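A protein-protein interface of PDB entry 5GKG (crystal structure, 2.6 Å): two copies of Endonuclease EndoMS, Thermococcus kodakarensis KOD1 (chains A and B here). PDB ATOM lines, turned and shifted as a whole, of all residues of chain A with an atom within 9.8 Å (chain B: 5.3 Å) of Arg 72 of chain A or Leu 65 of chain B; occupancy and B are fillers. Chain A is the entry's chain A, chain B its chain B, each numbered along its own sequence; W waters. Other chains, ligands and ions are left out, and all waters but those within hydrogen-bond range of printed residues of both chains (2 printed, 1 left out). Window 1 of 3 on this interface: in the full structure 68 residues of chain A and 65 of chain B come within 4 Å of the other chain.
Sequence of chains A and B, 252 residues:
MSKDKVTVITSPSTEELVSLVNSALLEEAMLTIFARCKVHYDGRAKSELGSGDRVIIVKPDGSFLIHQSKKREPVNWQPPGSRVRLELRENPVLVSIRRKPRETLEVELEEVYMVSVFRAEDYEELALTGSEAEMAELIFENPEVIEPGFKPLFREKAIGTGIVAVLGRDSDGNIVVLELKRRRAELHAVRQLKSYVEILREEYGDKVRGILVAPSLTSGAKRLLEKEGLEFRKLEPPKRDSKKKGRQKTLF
NZ of Lys 59 of chain A lies within hydrogen-bond range of ND1 of His 67 of chain B (3.0 Å).
The side-chain amino group (NZ) of Lys 59 of chain B sits at hydrogen-bond distance from a ring nitrogen (ND1) of His 67 of chain A (3.0 Å).
NZ of Lys 59 of chain B sits at hydrogen-bond distance from O of Gln 68 of chain A.
The side-chain amino group (NZ) of Lys 59 of chain B sits at hydrogen-bond distance from the backbone carbonyl oxygen (O) of Lys 70 of chain A (2.6 Å).
The backbone carbonyl oxygen (O) of Lys 71 of chain A lies within hydrogen-bond range of the side-chain amino group (NZ) of Lys 59 of chain B.
The backbone carbonyl oxygen (O) of Lys 71 of chain A sits at hydrogen-bond distance from the side-chain hydroxyl (OG) of Ser 63 of chain B (3.0 Å).
The side-chain carboxylate of Glu 73 of chain B lies within salt-bridge range of the guanidinium group of Arg 72 of chain A, at 3.0 Å.
O of Val 55 of chain A is in hydrogen-bond range of N of His 67 of chain A (2.8 Å).
N of Leu 65 of chain A is in hydrogen-bond range of O of Ile 57 of chain A, 2.7 Å away.
The guanidinium group (NH2) of Arg 72 of chain A is in salt-bridge range of the side-chain carboxylate (OE2) of Glu 73 of chain A, 2.8 Å away.
O of Val 55 of chain B is in hydrogen-bond range of N of His 67 of chain B (2.9 Å).
The backbone carbonyl oxygen (O) of Ile 57 of chain B sits at hydrogen-bond distance from the backbone NH (N) of Leu 65 of chain B.
Ile 57 of chain B touches Ile 57 of chain A.
Leu 65 of chain A touches His 67 of chain B (CD1 to NE2, 3.2 Å).
CE1 of His 67 of chain A touches CD1 of Leu 65 of chain B, 3.3 Å away.
Ser 69 of chain A touches Lys 59 of chain B.
Lys 71 of chain A touches Pro 80 of chain B (CA to CG, 3.7 Å).
OG of Ser 63 of chain B touches N of Arg 72 of chain A, at 3.9 Å.
Leu 65 of chain B touches Arg 72 of chain A (CD2 to O, 3.6 Å).
Arg 72 of chain A touches Pro 74 of chain B (NH1 to CG, 3.7 Å).
Trp 77 of chain B touches Arg 72 of chain A.
Lys 59 of chain B touches Glu 73 of chain A (NZ to O, 3.9 Å).
Printed residues of chain B within 4 Å of Leu 65 of chain A: His 67.
Printed residues of chain B within 4 Å of Gln 68 of chain A: Lys 59 (3.1 Å).
Arg 72 of chain A touches just these residues of chain B: Ser 63, Leu 65, Glu 73, Pro 74 and Trp 77.
Val 55 of chain B touches none of the printed residues of chain A.
Of the printed residues of chain A, His 67 of chain B touches Lys 59 (3.0 Å) and Leu 65 (3.2 Å).
Printed residues of chain A within 4 Å of Trp 77 of chain B: Arg 72 (3.1 Å).
Gln 78 of chain B touches none of the printed residues of chain A.
The nearest printed residue of chain B that does not touch Arg 72 of chain A is Gln 78 of chain B (4.2 Å).
Of the 16 printed residues of chain A, 10 touch a printed residue of chain B.
Hydrophobic or aromatic side chains of chain A within 4 Å of the printed part of chain B: Ile 57, Leu 65 and His 67.
Of the 17 printed residues of chain B, 9 touch a printed residue of chain A.
Hydrophobic or aromatic side chains of chain B within 4 Å of the printed part of chain A: Ile 57, Leu 65, His 67, Pro 74, Trp 77 and Pro 80.
Among the printed residues, Asp or Glu carboxylates within 4 Å of a Lys or Arg side-chain nitrogen of the other chain: Arg 72 of chain A with Glu 73 of chain B.
Ile 57 of chain A touches its own counterpart, Ile 57 of chain B.
Lys 59 of chain A touches His 67 of chain B, and with the chains exchanged His 67 of chain A touches Lys 59 of chain B.
Leu 65 of chain A touches His 67 of chain B, and with the chains exchanged His 67 of chain A touches Leu 65 of chain B.
Glu 73 of chain A touches Lys 59 of chain B, but with the chains exchanged Lys 59 of chain A does not touch Glu 73 of chain B (4.3 Å).
Positions printed for both chains: 55, 57, 59, 65, 66, 67, 73, 74, 76 and 77.
Water W1 lies within hydrogen-bond range of a ring nitrogen (NE2) of His 67 of chain B and a ring nitrogen (NE2) of His 67 of chain A.
Water W2 lies within hydrogen-bond range of O of Glu 73 of chain B and NZ of Lys 59 of chain A.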
ATOM      1  N   VAL A  55      30.324 -17.815  -6.004  1.00  0.00           N
ATOM      2  CA  VAL A  55      29.918 -17.397  -4.682  1.00  0.00           C
ATOM      3  C   VAL A  55      30.454 -18.380  -3.632  1.00  0.00           C
ATOM      4  O   VAL A  55      30.362 -19.602  -3.805  1.00  0.00           O
ATOM      5  CB  VAL A  55      28.400 -17.305  -4.572  1.00  0.00           C
ATOM      6  CG1 VAL A  55      27.991 -16.991  -3.119  1.00  0.00           C
ATOM      7  CG2 VAL A  55      27.883 -16.261  -5.544  1.00  0.00           C
ATOM      8  N   ILE A  57      30.374 -19.493   0.508  1.00  0.00           N
ATOM      9  CA  ILE A  57      29.677 -19.283   1.772  1.00  0.00           C
ATOM     10  C   ILE A  57      30.298 -20.149   2.857  1.00  0.00           C
ATOM     11  O   ILE A  57      30.537 -21.329   2.659  1.00  0.00           O
ATOM     12  CB  ILE A  57      28.177 -19.571   1.643  1.00  0.00           C
ATOM     13  CG1 ILE A  57      27.517 -18.477   0.816  1.00  0.00           C
ATOM     14  CG2 ILE A  57      27.499 -19.664   3.004  1.00  0.00           C
ATOM     15  CD1 ILE A  57      26.182 -18.897   0.332  1.00  0.00           C
ATOM     16  N   LYS A  59      29.563 -21.128   6.707  1.00  0.00           N
ATOM     17  CA  LYS A  59      28.605 -21.069   7.794  1.00  0.00           C
ATOM     18  C   LYS A  59      29.309 -21.142   9.140  1.00  0.00           C
ATOM     19  O   LYS A  59      30.428 -21.678   9.254  1.00  0.00           O
ATOM     20  CB  LYS A  59      27.586 -22.203   7.666  1.00  0.00           C
ATOM     21  CG  LYS A  59      26.754 -22.096   6.425  1.00  0.00           C
ATOM     22  CD  LYS A  59      25.587 -23.045   6.478  1.00  0.00           C
ATOM     23  CE  LYS A  59      24.826 -23.021   5.164  1.00  0.00           C
ATOM     24  NZ  LYS A  59      23.446 -23.504   5.423  1.00  0.00           N
ATOM     25  N   LEU A  65      30.573 -23.709   1.310  1.00  0.00           N
ATOM     26  CA  LEU A  65      29.893 -23.871   0.023  1.00  0.00           C
ATOM     27  C   LEU A  65      30.549 -23.071  -1.079  1.00  0.00           C
ATOM     28  O   LEU A  65      30.944 -21.921  -0.895  1.00  0.00           O
ATOM     29  CB  LEU A  65      28.435 -23.454   0.123  1.00  0.00           C
ATOM     30  CG  LEU A  65      27.541 -24.114   1.162  1.00  0.00           C
ATOM     31  CD1 LEU A  65      26.141 -23.554   1.036  1.00  0.00           C
ATOM     32  CD2 LEU A  65      27.520 -25.625   0.964  1.00  0.00           C
ATOM     33  N   ILE A  66      30.675 -23.677  -2.241  1.00  0.00           N
ATOM     34  CA  ILE A  66      31.169 -22.944  -3.388  1.00  0.00           C
ATOM     35  C   ILE A  66      30.210 -23.144  -4.560  1.00  0.00           C
ATOM     36  O   ILE A  66      30.001 -24.267  -5.030  1.00  0.00           O
ATOM     37  CB  ILE A  66      32.569 -23.386  -3.766  1.00  0.00           C
ATOM     38  CG1 ILE A  66      33.463 -23.380  -2.536  1.00  0.00           C
ATOM     39  CG2 ILE A  66      33.117 -22.521  -4.909  1.00  0.00           C
ATOM     40  CD1 ILE A  66      34.876 -23.803  -2.823  1.00  0.00           C
ATOM     41  N   HIS A  67      29.628 -22.052  -5.031  1.00  0.00           N
ATOM     42  CA  HIS A  67      28.604 -22.124  -6.072  1.00  0.00           C
ATOM     43  C   HIS A  67      28.996 -21.434  -7.366  1.00  0.00           C
ATOM     44  O   HIS A  67      29.339 -20.261  -7.383  1.00  0.00           O
ATOM     45  CB  HIS A  67      27.288 -21.529  -5.581  1.00  0.00           C
ATOM     46  CG  HIS A  67      26.478 -22.474  -4.756  1.00  0.00           C
ATOM     47  ND1 HIS A  67      25.758 -23.508  -5.308  1.00  0.00           N
ATOM     48  CD2 HIS A  67      26.284 -22.556  -3.418  1.00  0.00           C
ATOM     49  CE1 HIS A  67      25.145 -24.175  -4.349  1.00  0.00           C
ATOM     50  NE2 HIS A  67      25.449 -23.622  -3.191  1.00  0.00           N
ATOM     51  N   GLN A  68      28.942 -22.203  -8.445  1.00  0.00           N
ATOM     52  CA  GLN A  68      29.012 -21.679  -9.788  1.00  0.00           C
ATOM     53  C   GLN A  68      27.656 -21.065 -10.138  1.00  0.00           C
ATOM     54  O   GLN A  68      26.738 -21.069  -9.309  1.00  0.00           O
ATOM     55  CB  GLN A  68      29.413 -22.789 -10.755  1.00  0.00           C
ATOM     56  CG  GLN A  68      30.791 -23.324 -10.427  1.00  0.00           C
ATOM     57  CD  GLN A  68      31.381 -24.238 -11.486  1.00  0.00           C
ATOM     58  OE1 GLN A  68      32.297 -23.855 -12.200  1.00  0.00           O
ATOM     59  NE2 GLN A  68      30.897 -25.463 -11.551  1.00  0.00           N
ATOM     60  N   SER A  69      27.510 -20.522 -11.342  1.00  0.00           N
ATOM     61  CA  SER A  69      26.252 -19.850 -11.662  1.00  0.00           C
ATOM     62  C   SER A  69      25.198 -20.851 -12.159  1.00  0.00           C
ATOM     63  O   SER A  69      24.059 -20.501 -12.449  1.00  0.00           O
ATOM     64  CB  SER A  69      26.488 -18.734 -12.674  1.00  0.00           C
ATOM     65  OG  SER A  69      27.262 -19.205 -13.746  1.00  0.00           O
ATOM     66  N   LYS A  70      25.578 -22.115 -12.195  1.00  0.00           N
ATOM     67  CA  LYS A  70      24.647 -23.161 -12.546  1.00  0.00           C
ATOM     68  C   LYS A  70      24.487 -24.224 -11.464  1.00  0.00           C
ATOM     69  O   LYS A  70      25.300 -24.368 -10.541  1.00  0.00           O
ATOM     70  CB  LYS A  70      25.080 -23.808 -13.869  1.00  0.00           C
ATOM     71  CG  LYS A  70      24.535 -23.076 -15.084  1.00  0.00           C
ATOM     72  CD  LYS A  70      25.507 -23.069 -16.258  1.00  0.00           C
ATOM     73  CE  LYS A  70      26.008 -24.474 -16.574  1.00  0.00           C
ATOM     74  NZ  LYS A  70      24.909 -25.457 -16.846  1.00  0.00           N
ATOM     75  N   LYS A  71      23.415 -24.978 -11.666  1.00  0.00           N
ATOM     76  CA  LYS A  71      22.851 -26.079 -10.868  1.00  0.00           C
ATOM     77  C   LYS A  71      22.451 -25.809  -9.419  1.00  0.00           C
ATOM     78  O   LYS A  71      22.613 -24.697  -8.929  1.00  0.00           O
ATOM     79  CB  LYS A  71      23.891 -27.194 -10.843  1.00  0.00           C
ATOM     80  CG  LYS A  71      24.472 -27.580 -12.203  1.00  0.00           C
ATOM     81  CD  LYS A  71      23.596 -28.634 -12.885  1.00  0.00           C
ATOM     82  CE  LYS A  71      24.096 -28.968 -14.280  1.00  0.00           C
ATOM     83  NZ  LYS A  71      23.880 -27.833 -15.233  1.00  0.00           N
ATOM     84  N   ARG A  72      22.071 -26.858  -8.689  1.00  0.00           N
ATOM     85  CA  ARG A  72      21.590 -26.668  -7.324  1.00  0.00           C
ATOM     86  C   ARG A  72      22.661 -27.031  -6.318  1.00  0.00           C
ATOM     87  O   ARG A  72      22.628 -26.618  -5.153  1.00  0.00           O
ATOM     88  CB  ARG A  72      20.337 -27.505  -7.045  1.00  0.00           C
ATOM     89  CG  ARG A  72      19.637 -26.990  -5.795  1.00  0.00           C
ATOM     90  CD  ARG A  72      18.918 -28.024  -4.967  1.00  0.00           C
ATOM     91  NE  ARG A  72      19.812 -28.970  -4.344  1.00  0.00           N
ATOM     92  CZ  ARG A  72      19.541 -29.617  -3.212  1.00  0.00           C
ATOM     93  NH1 ARG A  72      18.409 -29.399  -2.555  1.00  0.00           N
ATOM     94  NH2 ARG A  72      20.425 -30.477  -2.721  1.00  0.00           N
ATOM     95  N   GLU A  73      23.626 -27.789  -6.813  1.00  0.00           N
ATOM     96  CA  GLU A  73      24.720 -28.309  -6.021  1.00  0.00           C
ATOM     97  C   GLU A  73      25.905 -27.372  -6.042  1.00  0.00           C
ATOM     98  O   GLU A  73      26.200 -26.766  -7.072  1.00  0.00           O
ATOM     99  CB  GLU A  73      25.134 -29.674  -6.548  1.00  0.00           C
ATOM    100  CG  GLU A  73      24.078 -30.720  -6.366  1.00  0.00           C
ATOM    101  CD  GLU A  73      23.619 -30.778  -4.928  1.00  0.00           C
ATOM    102  OE1 GLU A  73      24.453 -31.157  -4.077  1.00  0.00           O
ATOM    103  OE2 GLU A  73      22.441 -30.441  -4.650  1.00  0.00           O
ATOM    104  N   PRO A  74      26.579 -27.235  -4.894  1.00  0.00           N
ATOM    105  CA  PRO A  74      27.863 -26.538  -4.900  1.00  0.00           C
ATOM    106  C   PRO A  74      28.907 -27.336  -5.687  1.00  0.00           C
ATOM    107  O   PRO A  74      28.970 -28.552  -5.526  1.00  0.00           O
ATOM    108  CB  PRO A  74      28.233 -26.471  -3.406  1.00  0.00           C
ATOM    109  CG  PRO A  74      27.541 -27.664  -2.792  1.00  0.00           C
ATOM    110  CD  PRO A  74      26.231 -27.756  -3.559  1.00  0.00           C
ATOM    111  N   VAL A  75      29.728 -26.677  -6.491  1.00  0.00           N
ATOM    112  CA  VAL A  75      30.808 -27.375  -7.182  1.00  0.00           C
ATOM    113  C   VAL A  75      31.836 -28.019  -6.209  1.00  0.00           C
ATOM    114  O   VAL A  75      32.480 -29.001  -6.552  1.00  0.00           O
ATOM    115  CB  VAL A  75      31.548 -26.409  -8.147  1.00  0.00           C
ATOM    116  CG1 VAL A  75      32.186 -25.291  -7.361  1.00  0.00           C
ATOM    117  CG2 VAL A  75      32.610 -27.143  -8.958  1.00  0.00           C
ATOM    118  N   ASN A  76      32.023 -27.428  -5.027  1.00  0.00           N
ATOM    119  CA  ASN A  76      32.887 -27.972  -3.971  1.00  0.00           C
ATOM    120  C   ASN A  76      32.336 -27.515  -2.650  1.00  0.00           C
ATOM    121  O   ASN A  76      31.544 -26.572  -2.586  1.00  0.00           O
ATOM    122  CB  ASN A  76      34.351 -27.514  -4.077  1.00  0.00           C
ATOM    123  CG  ASN A  76      35.118 -28.226  -5.151  1.00  0.00           C
ATOM    124  OD1 ASN A  76      35.444 -27.635  -6.179  1.00  0.00           O
ATOM    125  ND2 ASN A  76      35.442 -29.500  -4.912  1.00  0.00           N
ATOM    126  N   TRP A  77      32.770 -28.166  -1.586  1.00  0.00           N
ATOM    127  CA  TRP A  77      32.173 -27.891  -0.301  1.00  0.00           C
ATOM    128  C   TRP A  77      32.971 -28.509   0.820  1.00  0.00           C
ATOM    129  O   TRP A  77      33.949 -29.232   0.602  1.00  0.00           O
ATOM    130  CB  TRP A  77      30.739 -28.428  -0.256  1.00  0.00           C
ATOM    131  CG  TRP A  77      30.688 -29.956  -0.312  1.00  0.00           C
ATOM    132  CD1 TRP A  77      30.643 -30.823   0.755  1.00  0.00           C
ATOM    133  CD2 TRP A  77      30.710 -30.776  -1.485  1.00  0.00           C
ATOM    134  NE1 TRP A  77      30.625 -32.118   0.317  1.00  0.00           N
ATOM    135  CE2 TRP A  77      30.675 -32.127  -1.048  1.00  0.00           C
ATOM    136  CE3 TRP A  77      30.770 -30.503  -2.862  1.00  0.00           C
ATOM    137  CZ2 TRP A  77      30.697 -33.201  -1.935  1.00  0.00           C
ATOM    138  CZ3 TRP A  77      30.779 -31.576  -3.746  1.00  0.00           C
ATOM    139  CH2 TRP A  77      30.729 -32.912  -3.274  1.00  0.00           C
ATOM    140  N   VAL B  55      20.225 -16.703   3.974  1.00  0.00           N
ATOM    141  CA  VAL B  55      20.861 -16.286   2.735  1.00  0.00           C
ATOM    142  C   VAL B  55      20.046 -16.854   1.593  1.00  0.00           C
ATOM    143  O   VAL B  55      19.728 -18.038   1.592  1.00  0.00           O
ATOM    144  CB  VAL B  55      22.312 -16.790   2.630  1.00  0.00           C
ATOM    145  CG1 VAL B  55      22.893 -16.459   1.262  1.00  0.00           C
ATOM    146  CG2 VAL B  55      23.135 -16.215   3.736  1.00  0.00           C
ATOM    147  N   ILE B  56      19.684 -16.010   0.636  1.00  0.00           N
ATOM    148  CA  ILE B  56      18.934 -16.460  -0.530  1.00  0.00           C
ATOM    149  C   ILE B  56      19.773 -16.272  -1.798  1.00  0.00           C
ATOM    150  O   ILE B  56      20.428 -15.243  -1.976  1.00  0.00           O
ATOM    151  CB  ILE B  56      17.613 -15.719  -0.620  1.00  0.00           C
ATOM    152  CG1 ILE B  56      16.885 -15.892   0.703  1.00  0.00           C
ATOM    153  CG2 ILE B  56      16.759 -16.247  -1.768  1.00  0.00           C
ATOM    154  CD1 ILE B  56      15.671 -15.036   0.854  1.00  0.00           C
ATOM    155  N   ILE B  57      19.803 -17.294  -2.652  1.00  0.00           N
ATOM    156  CA  ILE B  57      20.547 -17.221  -3.914  1.00  0.00           C
ATOM    157  C   ILE B  57      19.662 -17.699  -5.088  1.00  0.00           C
ATOM    158  O   ILE B  57      19.039 -18.765  -5.021  1.00  0.00           O
ATOM    159  CB  ILE B  57      21.855 -18.045  -3.852  1.00  0.00           C
ATOM    160  CG1 ILE B  57      22.781 -17.489  -2.774  1.00  0.00           C
ATOM    161  CG2 ILE B  57      22.575 -18.058  -5.207  1.00  0.00           C
ATOM    162  CD1 ILE B  57      24.074 -18.298  -2.577  1.00  0.00           C
ATOM    163  N   VAL B  58      19.567 -16.876  -6.133  1.00  0.00           N
ATOM    164  CA  VAL B  58      18.895 -17.261  -7.366  1.00  0.00           C
ATOM    165  C   VAL B  58      19.932 -17.249  -8.456  1.00  0.00           C
ATOM    166  O   VAL B  58      20.514 -16.203  -8.747  1.00  0.00           O
ATOM    167  CB  VAL B  58      17.735 -16.318  -7.766  1.00  0.00           C
ATOM    168  CG1 VAL B  58      17.106 -16.805  -9.065  1.00  0.00           C
ATOM    169  CG2 VAL B  58      16.687 -16.269  -6.690  1.00  0.00           C
ATOM    170  N   LYS B  59      20.186 -18.415  -9.044  1.00  0.00           N
ATOM    171  CA  LYS B  59      21.180 -18.509 -10.109  1.00  0.00           C
ATOM    172  C   LYS B  59      20.510 -18.181 -11.453  1.00  0.00           C
ATOM    173  O   LYS B  59      19.292 -18.351 -11.594  1.00  0.00           O
ATOM    174  CB  LYS B  59      21.831 -19.898 -10.148  1.00  0.00           C
ATOM    175  CG  LYS B  59      22.391 -20.417  -8.831  1.00  0.00           C
ATOM    176  CD  LYS B  59      23.492 -21.422  -9.126  1.00  0.00           C
ATOM    177  CE  LYS B  59      24.014 -22.086  -7.874  1.00  0.00           C
ATOM    178  NZ  LYS B  59      24.893 -23.274  -8.214  1.00  0.00           N
ATOM    179  N   SER B  63      18.110 -22.040 -10.630  1.00  0.00           N
ATOM    180  CA  SER B  63      18.351 -22.697  -9.345  1.00  0.00           C
ATOM    181  C   SER B  63      18.105 -21.701  -8.232  1.00  0.00           C
ATOM    182  O   SER B  63      18.581 -20.575  -8.277  1.00  0.00           O
ATOM    183  CB  SER B  63      19.765 -23.253  -9.261  1.00  0.00           C
ATOM    184  OG  SER B  63      20.024 -24.066 -10.388  1.00  0.00           O
ATOM    185  N   PHE B  64      17.351 -22.125  -7.236  1.00  0.00           N
ATOM    186  CA  PHE B  64      16.998 -21.259  -6.132  1.00  0.00           C
ATOM    187  C   PHE B  64      17.466 -21.940  -4.824  1.00  0.00           C
ATOM    188  O   PHE B  64      17.183 -23.108  -4.603  1.00  0.00           O
ATOM    189  CB  PHE B  64      15.487 -20.999  -6.187  1.00  0.00           C
ATOM    190  CG  PHE B  64      14.996 -19.886  -5.309  1.00  0.00           C
ATOM    191  CD1 PHE B  64      15.218 -19.892  -3.943  1.00  0.00           C
ATOM    192  CD2 PHE B  64      14.223 -18.877  -5.842  1.00  0.00           C
ATOM    193  CE1 PHE B  64      14.704 -18.890  -3.134  1.00  0.00           C
ATOM    194  CE2 PHE B  64      13.715 -17.876  -5.044  1.00  0.00           C
ATOM    195  CZ  PHE B  64      13.942 -17.889  -3.689  1.00  0.00           C
ATOM    196  N   LEU B  65      18.197 -21.211  -3.980  1.00  0.00           N
ATOM    197  CA  LEU B  65      18.703 -21.734  -2.699  1.00  0.00           C
ATOM    198  C   LEU B  65      18.285 -20.893  -1.486  1.00  0.00           C
ATOM    199  O   LEU B  65      18.355 -19.665  -1.503  1.00  0.00           O
ATOM    200  CB  LEU B  65      20.231 -21.815  -2.738  1.00  0.00           C
ATOM    201  CG  LEU B  65      20.871 -22.603  -3.888  1.00  0.00           C
ATOM    202  CD1 LEU B  65      22.356 -22.477  -3.835  1.00  0.00           C
ATOM    203  CD2 LEU B  65      20.460 -24.051  -3.807  1.00  0.00           C
ATOM    204  N   ILE B  66      17.837 -21.543  -0.429  1.00  0.00           N
ATOM    205  CA  ILE B  66      17.684 -20.844   0.843  1.00  0.00           C
ATOM    206  C   ILE B  66      18.492 -21.538   1.954  1.00  0.00           C
ATOM    207  O   ILE B  66      18.203 -22.674   2.337  1.00  0.00           O
ATOM    208  CB  ILE B  66      16.224 -20.747   1.264  1.00  0.00           C
ATOM    209  CG1 ILE B  66      15.407 -20.106   0.151  1.00  0.00           C
ATOM    210  CG2 ILE B  66      16.100 -19.955   2.577  1.00  0.00           C
ATOM    211  CD1 ILE B  66      13.934 -20.329   0.295  1.00  0.00           C
ATOM    212  N   HIS B  67      19.487 -20.825   2.474  1.00  0.00           N
ATOM    213  CA  HIS B  67      20.368 -21.354   3.511  1.00  0.00           C
ATOM    214  C   HIS B  67      20.228 -20.733   4.901  1.00  0.00           C
ATOM    215  O   HIS B  67      20.291 -19.522   5.081  1.00  0.00           O
ATOM    216  CB  HIS B  67      21.818 -21.210   3.068  1.00  0.00           C
ATOM    217  CG  HIS B  67      22.270 -22.311   2.177  1.00  0.00           C
ATOM    218  ND1 HIS B  67      22.416 -23.609   2.618  1.00  0.00           N
ATOM    219  CD2 HIS B  67      22.595 -22.321   0.864  1.00  0.00           C
ATOM    220  CE1 HIS B  67      22.825 -24.365   1.617  1.00  0.00           C
ATOM    221  NE2 HIS B  67      22.930 -23.610   0.541  1.00  0.00           N
ATOM    222  N   GLU B  73      23.066 -28.642   3.343  1.00  0.00           N
ATOM    223  CA  GLU B  73      21.873 -28.556   2.525  1.00  0.00           C
ATOM    224  C   GLU B  73      21.132 -27.235   2.695  1.00  0.00           C
ATOM    225  O   GLU B  73      21.055 -26.677   3.791  1.00  0.00           O
ATOM    226  CB  GLU B  73      20.950 -29.735   2.845  1.00  0.00           C
ATOM    227  CG  GLU B  73      21.540 -31.039   2.397  1.00  0.00           C
ATOM    228  CD  GLU B  73      22.215 -30.897   1.056  1.00  0.00           C
ATOM    229  OE1 GLU B  73      21.479 -30.705   0.056  1.00  0.00           O
ATOM    230  OE2 GLU B  73      23.475 -30.930   1.006  1.00  0.00           O
ATOM    231  N   PRO B  74      20.578 -26.725   1.600  1.00  0.00           N
ATOM    232  CA  PRO B  74      19.603 -25.631   1.725  1.00  0.00           C
ATOM    233  C   PRO B  74      18.350 -26.096   2.478  1.00  0.00           C
ATOM    234  O   PRO B  74      17.936 -27.242   2.300  1.00  0.00           O
ATOM    235  CB  PRO B  74      19.275 -25.286   0.267  1.00  0.00           C
ATOM    236  CG  PRO B  74      19.558 -26.546  -0.500  1.00  0.00           C
ATOM    237  CD  PRO B  74      20.767 -27.158   0.207  1.00  0.00           C
ATOM    238  N   ASN B  76      15.476 -24.954   1.853  1.00  0.00           N
ATOM    239  CA  ASN B  76      14.518 -25.025   0.771  1.00  0.00           C
ATOM    240  C   ASN B  76      15.230 -24.646  -0.505  1.00  0.00           C
ATOM    241  O   ASN B  76      16.300 -24.021  -0.485  1.00  0.00           O
ATOM    242  CB  ASN B  76      13.330 -24.096   0.992  1.00  0.00           C
ATOM    243  CG  ASN B  76      12.279 -24.687   1.902  1.00  0.00           C
ATOM    244  OD1 ASN B  76      12.044 -24.175   2.998  1.00  0.00           O
ATOM    245  ND2 ASN B  76      11.619 -25.755   1.445  1.00  0.00           N
ATOM    246  N   TRP B  77      14.638 -25.015  -1.625  1.00  0.00           N
ATOM    247  CA  TRP B  77      15.315 -24.810  -2.874  1.00  0.00           C
ATOM    248  C   TRP B  77      14.346 -24.933  -4.039  1.00  0.00           C
ATOM    249  O   TRP B  77      13.163 -25.237  -3.868  1.00  0.00           O
ATOM    250  CB  TRP B  77      16.446 -25.833  -3.023  1.00  0.00           C
ATOM    251  CG  TRP B  77      15.938 -27.233  -3.119  1.00  0.00           C
ATOM    252  CD1 TRP B  77      15.651 -27.924  -4.262  1.00  0.00           C
ATOM    253  CD2 TRP B  77      15.618 -28.114  -2.032  1.00  0.00           C
ATOM    254  NE1 TRP B  77      15.184 -29.182  -3.956  1.00  0.00           N
ATOM    255  CE2 TRP B  77      15.151 -29.325  -2.597  1.00  0.00           C
ATOM    256  CE3 TRP B  77      15.699 -28.011  -0.641  1.00  0.00           C
ATOM    257  CZ2 TRP B  77      14.757 -30.412  -1.817  1.00  0.00           C
ATOM    258  CZ3 TRP B  77      15.296 -29.092   0.128  1.00  0.00           C
ATOM    259  CH2 TRP B  77      14.827 -30.278  -0.468  1.00  0.00           C
ATOM    260  N   GLN B  78      14.878 -24.715  -5.227  1.00  0.00           N
ATOM    261  CA  GLN B  78      14.170 -24.999  -6.450  1.00  0.00           C
ATOM    262  C   GLN B  78      15.262 -25.398  -7.426  1.00  0.00           C
ATOM    263  O   GLN B  78      16.356 -24.852  -7.365  1.00  0.00           O
ATOM    264  CB  GLN B  78      13.379 -23.764  -6.901  1.00  0.00           C
ATOM    265  CG  GLN B  78      12.051 -23.985  -7.558  1.00  0.00           C
ATOM    266  CD  GLN B  78      11.024 -24.680  -6.709  1.00  0.00           C
ATOM    267  OE1 GLN B  78      11.163 -25.852  -6.384  1.00  0.00           O
ATOM    268  NE2 GLN B  78       9.944 -23.982  -6.407  1.00  0.00           N
ATOM    269  N   PRO B  79      14.989 -26.376  -8.306  1.00  0.00           N
ATOM    270  CA  PRO B  79      15.981 -26.893  -9.256  1.00  0.00           C
ATOM    271  C   PRO B  79      16.187 -26.017 -10.478  1.00  0.00           C
ATOM    272  O   PRO B  79      15.329 -25.173 -10.773  1.00  0.00           O
ATOM    273  CB  PRO B  79      15.384 -28.241  -9.673  1.00  0.00           C
ATOM    274  CG  PRO B  79      13.948 -28.036  -9.580  1.00  0.00           C
ATOM    275  CD  PRO B  79      13.729 -27.138  -8.379  1.00  0.00           C
ATOM    276  N   PRO B  80      17.291 -26.243 -11.209  1.00  0.00           N
ATOM    277  CA  PRO B  80      17.496 -25.514 -12.458  1.00  0.00           C
ATOM    278  C   PRO B  80      16.246 -25.549 -13.341  1.00  0.00           C
ATOM    279  O   PRO B  80      15.478 -26.525 -13.347  1.00  0.00           O
ATOM    280  CB  PRO B  80      18.665 -26.253 -13.112  1.00  0.00           C
ATOM    281  CG  PRO B  80      19.430 -26.819 -11.981  1.00  0.00           C
ATOM    282  CD  PRO B  80      18.422 -27.129 -10.888  1.00  0.00           C
HETATM  283  O   HOH W   1      23.795 -25.273  -1.539  1.00  0.00           O
HETATM  284  O   HOH W   2      20.213 -24.347   5.502  1.00  0.00           O
